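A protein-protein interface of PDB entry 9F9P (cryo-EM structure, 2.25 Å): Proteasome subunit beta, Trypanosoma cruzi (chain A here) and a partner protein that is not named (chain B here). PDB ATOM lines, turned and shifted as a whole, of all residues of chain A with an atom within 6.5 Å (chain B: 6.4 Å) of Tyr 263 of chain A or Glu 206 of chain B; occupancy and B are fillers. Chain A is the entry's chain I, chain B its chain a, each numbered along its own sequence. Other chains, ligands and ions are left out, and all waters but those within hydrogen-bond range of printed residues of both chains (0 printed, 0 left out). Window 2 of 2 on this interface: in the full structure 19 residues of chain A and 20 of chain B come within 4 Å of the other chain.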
ATOM      1  N   ARG A 261     -25.095  25.410  -1.172  1.00  0.00           N
ATOM      2  CA  ARG A 261     -23.719  25.095  -1.528  1.00  0.00           C
ATOM      3  C   ARG A 261     -23.437  25.556  -2.963  1.00  0.00           C
ATOM      4  O   ARG A 261     -24.267  25.378  -3.857  1.00  0.00           O
ATOM      5  CB  ARG A 261     -23.465  23.594  -1.321  1.00  0.00           C
ATOM      6  CG  ARG A 261     -22.690  23.254  -0.053  1.00  0.00           C
ATOM      7  CD  ARG A 261     -21.206  23.292  -0.355  1.00  0.00           C
ATOM      8  NE  ARG A 261     -20.296  23.234   0.781  1.00  0.00           N
ATOM      9  CZ  ARG A 261     -20.081  22.165   1.539  1.00  0.00           C
ATOM     10  NH1 ARG A 261     -20.920  21.146   1.497  1.00  0.00           N
ATOM     11  NH2 ARG A 261     -19.055  22.140   2.376  1.00  0.00           N
ATOM     12  N   LYS A 262     -22.250  26.155  -3.157  1.00  0.00           N
ATOM     13  CA  LYS A 262     -21.814  26.699  -4.438  1.00  0.00           C
ATOM     14  C   LYS A 262     -20.915  25.685  -5.152  1.00  0.00           C
ATOM     15  O   LYS A 262     -21.108  25.400  -6.335  1.00  0.00           O
ATOM     16  CB  LYS A 262     -21.093  28.036  -4.217  1.00  0.00           C
ATOM     17  CG  LYS A 262     -21.848  29.030  -3.339  1.00  0.00           C
ATOM     18  CD  LYS A 262     -21.572  30.493  -3.631  1.00  0.00           C
ATOM     19  CE  LYS A 262     -22.784  31.372  -3.386  1.00  0.00           C
ATOM     20  NZ  LYS A 262     -22.541  32.784  -3.764  1.00  0.00           N
ATOM     21  N   TYR A 263     -19.930  25.163  -4.405  1.00  0.00           N
ATOM     22  CA  TYR A 263     -18.994  24.143  -4.857  1.00  0.00           C
ATOM     23  C   TYR A 263     -19.283  22.853  -4.083  1.00  0.00           C
ATOM     24  O   TYR A 263     -19.171  22.843  -2.858  1.00  0.00           O
ATOM     25  CB  TYR A 263     -17.571  24.676  -4.636  1.00  0.00           C
ATOM     26  CG  TYR A 263     -16.396  23.893  -5.193  1.00  0.00           C
ATOM     27  CD1 TYR A 263     -16.087  23.893  -6.552  1.00  0.00           C
ATOM     28  CD2 TYR A 263     -15.524  23.226  -4.338  1.00  0.00           C
ATOM     29  CE1 TYR A 263     -14.981  23.209  -7.047  1.00  0.00           C
ATOM     30  CE2 TYR A 263     -14.421  22.534  -4.817  1.00  0.00           C
ATOM     31  CZ  TYR A 263     -14.145  22.521  -6.176  1.00  0.00           C
ATOM     32  OH  TYR A 263     -13.034  21.828  -6.622  1.00  0.00           O
ATOM     33  N   PRO A 264     -19.661  21.727  -4.750  1.00  0.00           N
ATOM     34  CA  PRO A 264     -19.979  20.477  -4.047  1.00  0.00           C
ATOM     35  C   PRO A 264     -18.828  19.898  -3.219  1.00  0.00           C
ATOM     36  O   PRO A 264     -17.669  19.931  -3.637  1.00  0.00           O
ATOM     37  CB  PRO A 264     -20.364  19.497  -5.171  1.00  0.00           C
ATOM     38  CG  PRO A 264     -19.738  20.090  -6.417  1.00  0.00           C
ATOM     39  CD  PRO A 264     -19.798  21.590  -6.209  1.00  0.00           C
ATOM     40  N   LYS A 265     -19.174  19.352  -2.046  1.00  0.00           N
ATOM     41  CA  LYS A 265     -18.190  18.859  -1.095  1.00  0.00           C
ATOM     42  C   LYS A 265     -17.384  17.722  -1.726  1.00  0.00           C
ATOM     43  O   LYS A 265     -17.938  16.704  -2.137  1.00  0.00           O
ATOM     44  CB  LYS A 265     -18.865  18.434   0.218  1.00  0.00           C
ATOM     45  CG  LYS A 265     -17.923  17.802   1.244  1.00  0.00           C
ATOM     46  CD  LYS A 265     -18.129  18.215   2.696  1.00  0.00           C
ATOM     47  CE  LYS A 265     -19.125  17.378   3.467  1.00  0.00           C
ATOM     48  NZ  LYS A 265     -18.997  17.610   4.929  1.00  0.00           N
ATOM     49  N   GLN A 266     -16.065  17.932  -1.815  1.00  0.00           N
ATOM     50  CA  GLN A 266     -15.136  16.880  -2.194  1.00  0.00           C
ATOM     51  C   GLN A 266     -15.200  15.795  -1.122  1.00  0.00           C
ATOM     52  O   GLN A 266     -15.248  16.088   0.069  1.00  0.00           O
ATOM     53  CB  GLN A 266     -13.714  17.437  -2.350  1.00  0.00           C
ATOM     54  CG  GLN A 266     -12.746  16.505  -3.079  1.00  0.00           C
ATOM     55  CD  GLN A 266     -11.309  16.967  -2.987  1.00  0.00           C
ATOM     56  OE1 GLN A 266     -10.426  16.229  -2.558  1.00  0.00           O
ATOM     57  NE2 GLN A 266     -11.062  18.207  -3.385  1.00  0.00           N
ATOM     58  N   MET B 201      -0.592  20.628  -9.777  1.00  0.00           N
ATOM     59  CA  MET B 201      -1.137  21.964  -9.626  1.00  0.00           C
ATOM     60  C   MET B 201      -2.658  21.914  -9.457  1.00  0.00           C
ATOM     61  O   MET B 201      -3.177  22.559  -8.553  1.00  0.00           O
ATOM     62  CB  MET B 201      -0.785  22.835 -10.837  1.00  0.00           C
ATOM     63  CG  MET B 201      -0.071  24.113 -10.491  1.00  0.00           C
ATOM     64  SD  MET B 201       0.960  24.787 -11.849  1.00  0.00           S
ATOM     65  CE  MET B 201      -0.256  24.995 -13.152  1.00  0.00           C
ATOM     66  N   THR B 202      -3.336  21.109 -10.287  1.00  0.00           N
ATOM     67  CA  THR B 202      -4.791  21.060 -10.373  1.00  0.00           C
ATOM     68  C   THR B 202      -5.432  20.476  -9.116  1.00  0.00           C
ATOM     69  O   THR B 202      -6.438  20.973  -8.606  1.00  0.00           O
ATOM     70  CB  THR B 202      -5.203  20.274 -11.622  1.00  0.00           C
ATOM     71  OG1 THR B 202      -5.013  21.159 -12.733  1.00  0.00           O
ATOM     72  CG2 THR B 202      -6.646  19.806 -11.599  1.00  0.00           C
ATOM     73  N   GLU B 203      -4.797  19.440  -8.606  1.00  0.00           N
ATOM     74  CA  GLU B 203      -5.257  18.682  -7.464  1.00  0.00           C
ATOM     75  C   GLU B 203      -5.000  19.485  -6.188  1.00  0.00           C
ATOM     76  O   GLU B 203      -5.803  19.474  -5.266  1.00  0.00           O
ATOM     77  CB  GLU B 203      -4.521  17.355  -7.619  1.00  0.00           C
ATOM     78  CG  GLU B 203      -4.839  16.248  -6.649  1.00  0.00           C
ATOM     79  CD  GLU B 203      -4.300  14.902  -7.148  1.00  0.00           C
ATOM     80  OE1 GLU B 203      -3.176  14.880  -7.738  1.00  0.00           O
ATOM     81  OE2 GLU B 203      -4.995  13.865  -6.950  1.00  0.00           O
ATOM     82  N   THR B 204      -3.885  20.206  -6.144  1.00  0.00           N
ATOM     83  CA  THR B 204      -3.549  21.082  -5.032  1.00  0.00           C
ATOM     84  C   THR B 204      -4.522  22.254  -4.931  1.00  0.00           C
ATOM     85  O   THR B 204      -4.954  22.590  -3.836  1.00  0.00           O
ATOM     86  CB  THR B 204      -2.107  21.575  -5.129  1.00  0.00           C
ATOM     87  OG1 THR B 204      -1.231  20.450  -5.050  1.00  0.00           O
ATOM     88  CG2 THR B 204      -1.760  22.498  -3.988  1.00  0.00           C
ATOM     89  N   LEU B 205      -4.890  22.840  -6.068  1.00  0.00           N
ATOM     90  CA  LEU B 205      -5.860  23.919  -6.099  1.00  0.00           C
ATOM     91  C   LEU B 205      -7.247  23.437  -5.663  1.00  0.00           C
ATOM     92  O   LEU B 205      -7.985  24.202  -5.065  1.00  0.00           O
ATOM     93  CB  LEU B 205      -5.894  24.517  -7.502  1.00  0.00           C
ATOM     94  CG  LEU B 205      -6.923  25.632  -7.681  1.00  0.00           C
ATOM     95  CD1 LEU B 205      -6.656  26.794  -6.735  1.00  0.00           C
ATOM     96  CD2 LEU B 205      -6.965  26.127  -9.104  1.00  0.00           C
ATOM     97  N   GLU B 206      -7.603  22.179  -5.890  1.00  0.00           N
ATOM     98  CA  GLU B 206      -8.907  21.671  -5.471  1.00  0.00           C
ATOM     99  C   GLU B 206      -8.967  21.457  -3.959  1.00  0.00           C
ATOM    100  O   GLU B 206     -10.000  21.672  -3.339  1.00  0.00           O
ATOM    101  CB  GLU B 206      -9.252  20.370  -6.184  1.00  0.00           C
ATOM    102  CG  GLU B 206      -9.850  20.610  -7.550  1.00  0.00           C
ATOM    103  CD  GLU B 206      -9.949  19.373  -8.445  1.00  0.00           C
ATOM    104  OE1 GLU B 206      -9.420  18.287  -8.056  1.00  0.00           O
ATOM    105  OE2 GLU B 206     -10.552  19.493  -9.553  1.00  0.00           O
ATOM    106  N   MET B 207      -7.853  21.073  -3.368  1.00  0.00           N
ATOM    107  CA  MET B 207      -7.805  20.910  -1.943  1.00  0.00           C
ATOM    108  C   MET B 207      -8.006  22.272  -1.256  1.00  0.00           C
ATOM    109  O   MET B 207      -8.708  22.370  -0.255  1.00  0.00           O
ATOM    110  CB  MET B 207      -6.467  20.249  -1.591  1.00  0.00           C
ATOM    111  CG  MET B 207      -6.081  20.278  -0.136  1.00  0.00           C
ATOM    112  SD  MET B 207      -4.596  19.264   0.247  1.00  0.00           S
ATOM    113  CE  MET B 207      -4.826  17.852  -0.841  1.00  0.00           C
ATOM    114  N   LEU B 208      -7.397  23.346  -1.768  1.00  0.00           N
ATOM    115  CA  LEU B 208      -7.553  24.637  -1.130  1.00  0.00           C
ATOM    116  C   LEU B 208      -8.978  25.144  -1.316  1.00  0.00           C
ATOM    117  O   LEU B 208      -9.474  25.806  -0.424  1.00  0.00           O
ATOM    118  CB  LEU B 208      -6.580  25.660  -1.712  1.00  0.00           C
ATOM    119  CG  LEU B 208      -5.147  25.565  -1.237  1.00  0.00           C
ATOM    120  CD1 LEU B 208      -4.262  26.514  -2.037  1.00  0.00           C
ATOM    121  CD2 LEU B 208      -5.029  25.867   0.239  1.00  0.00           C
ATOM    122  N   LYS B 209      -9.598  24.909  -2.479  1.00  0.00           N
ATOM    123  CA  LYS B 209     -10.988  25.306  -2.674  1.00  0.00           C
ATOM    124  C   LYS B 209     -11.895  24.670  -1.618  1.00  0.00           C
ATOM    125  O   LYS B 209     -12.794  25.313  -1.093  1.00  0.00           O
ATOM    126  CB  LYS B 209     -11.522  24.942  -4.059  1.00  0.00           C
ATOM    127  CG  LYS B 209     -11.082  25.912  -5.139  1.00  0.00           C
ATOM    128  CD  LYS B 209     -11.360  25.483  -6.557  1.00  0.00           C
ATOM    129  CE  LYS B 209     -10.801  26.512  -7.519  1.00  0.00           C
ATOM    130  NZ  LYS B 209     -11.079  26.146  -8.921  1.00  0.00           N
ATOM    131  N   ASN B 210     -11.623  23.423  -1.293  1.00  0.00           N
ATOM    132  CA  ASN B 210     -12.443  22.703  -0.352  1.00  0.00           C
ATOM    133  C   ASN B 210     -12.145  23.179   1.087  1.00  0.00           C
ATOM    134  O   ASN B 210     -13.030  23.248   1.938  1.00  0.00           O
ATOM    135  CB  ASN B 210     -12.276  21.224  -0.672  1.00  0.00           C
ATOM    136  CG  ASN B 210     -13.243  20.357   0.091  1.00  0.00           C
ATOM    137  OD1 ASN B 210     -14.424  20.296  -0.251  1.00  0.00           O
ATOM    138  ND2 ASN B 210     -12.752  19.705   1.139  1.00  0.00           N
ATOM    139  N   ALA B 211     -10.902  23.528   1.397  1.00  0.00           N
ATOM    140  CA  ALA B 211     -10.579  24.034   2.716  1.00  0.00           C
ATOM    141  C   ALA B 211     -11.207  25.408   3.005  1.00  0.00           C
ATOM    142  O   ALA B 211     -11.568  25.712   4.144  1.00  0.00           O
ATOM    143  CB  ALA B 211      -9.093  24.144   2.825  1.00  0.00           C
ATOM    144  N   THR B 213     -13.981  26.547   1.507  1.00  0.00           N
ATOM    145  CA  THR B 213     -15.421  26.336   1.574  1.00  0.00           C
ATOM    146  C   THR B 213     -15.835  25.901   2.990  1.00  0.00           C
ATOM    147  O   THR B 213     -16.709  26.507   3.594  1.00  0.00           O
ATOM    148  CB  THR B 213     -15.852  25.351   0.487  1.00  0.00           C
ATOM    149  OG1 THR B 213     -15.652  25.905  -0.817  1.00  0.00           O
ATOM    150  CG2 THR B 213     -17.314  25.018   0.616  1.00  0.00           C
ATOM    151  N   PHE B 241     -12.885  32.755  -6.752  1.00  0.00           N
ATOM    152  CA  PHE B 241     -13.739  31.639  -6.368  1.00  0.00           C
ATOM    153  C   PHE B 241     -14.775  32.106  -5.347  1.00  0.00           C
ATOM    154  O   PHE B 241     -14.394  32.646  -4.325  1.00  0.00           O
ATOM    155  CB  PHE B 241     -12.821  30.517  -5.892  1.00  0.00           C
ATOM    156  CG  PHE B 241     -13.481  29.297  -5.300  1.00  0.00           C
ATOM    157  CD1 PHE B 241     -14.184  28.403  -6.096  1.00  0.00           C
ATOM    158  CD2 PHE B 241     -13.416  29.052  -3.925  1.00  0.00           C
ATOM    159  CE1 PHE B 241     -14.790  27.279  -5.537  1.00  0.00           C
ATOM    160  CE2 PHE B 241     -14.020  27.927  -3.361  1.00  0.00           C
ATOM    161  CZ  PHE B 241     -14.709  27.037  -4.174  1.00  0.00           C
ATOM    162  N   GLU B 242     -16.080  31.908  -5.614  1.00  0.00           N
ATOM    163  CA  GLU B 242     -17.168  32.307  -4.708  1.00  0.00           C
ATOM    164  C   GLU B 242     -17.343  31.416  -3.458  1.00  0.00           C
ATOM    165  O   GLU B 242     -17.154  30.199  -3.487  1.00  0.00           O
ATOM    166  CB  GLU B 242     -18.502  32.298  -5.437  1.00  0.00           C
ATOM    167  CG  GLU B 242     -18.513  33.132  -6.719  1.00  0.00           C
ATOM    168  CD  GLU B 242     -18.248  34.628  -6.594  1.00  0.00           C
ATOM    169  OE1 GLU B 242     -19.081  35.329  -5.961  1.00  0.00           O
ATOM    170  OE2 GLU B 242     -17.214  35.102  -7.144  1.00  0.00           O
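The side-chain amide oxygen (OD1) of Asn 210 of chain B lies within hydrogen-bond range of the backbone NH (N) of Gln 266 of chain A (3.3 Å).
The backbone carbonyl oxygen of Lys 209 of chain B lies within hydrogen-bond range of the side-chain hydroxyl of Thr 213 of chain B (2.9 Å).
NE of Arg 261 of chain A touches CG2 of Thr 213 of chain B, at 3.5 Å. Glu 242 of chain B touches Lys 262 of chain A. Tyr 263 of chain A touches Glu 206 of chain B. Lys 209 of chain B touches Tyr 263 of chain A. Tyr 263 of chain A touches Phe 241 of chain B. Gln 266 of chain A touches Glu 206 of chain B (NE2 to O, 3.6 Å).
Tyr 263 of chain A touches three residues of chain B. Glu 206 of chain B touches just these residues of chain A: Tyr 263 and Gln 266. Printed residues of chain B within 4 Å of Arg 261 of chain A: Thr 213. Printed residues of chain A within 4 Å of Phe 241 of chain B: Tyr 263. Of the printed residues of chain A, Lys 209 of chain B touches Tyr 263 (3.8 Å). Of the printed residues of chain A, Asn 210 of chain B touches Gln 266 (3.3 Å). Met 207 of chain B touches none of the printed residues of chain A. Pro 264 of chain A touches none of the printed residues of chain B. The nearest residue of chain B that does not touch Tyr 263 of chain A is Thr 213 of chain B (4.4 Å). The nearest printed residue of chain B that does not touch Gln 266 of chain A is Met 207 of chain B (4.3 Å).
Printed residues of chain B that touch a printed residue of chain A: Glu 206, Lys 209, Asn 210, Thr 213, Phe 241 and Glu 242. Printed residues of chain A that touch a printed residue of chain B: Arg 261, Lys 262, Tyr 263 and Gln 266. Hydrophobic or aromatic side chains of chain A that line the printed part of chain B: Tyr 263. Along chain A the printed residues that touch a printed residue of chain B span positions 261 to 266. Among the printed residues, 7 pairs touch across the chains.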
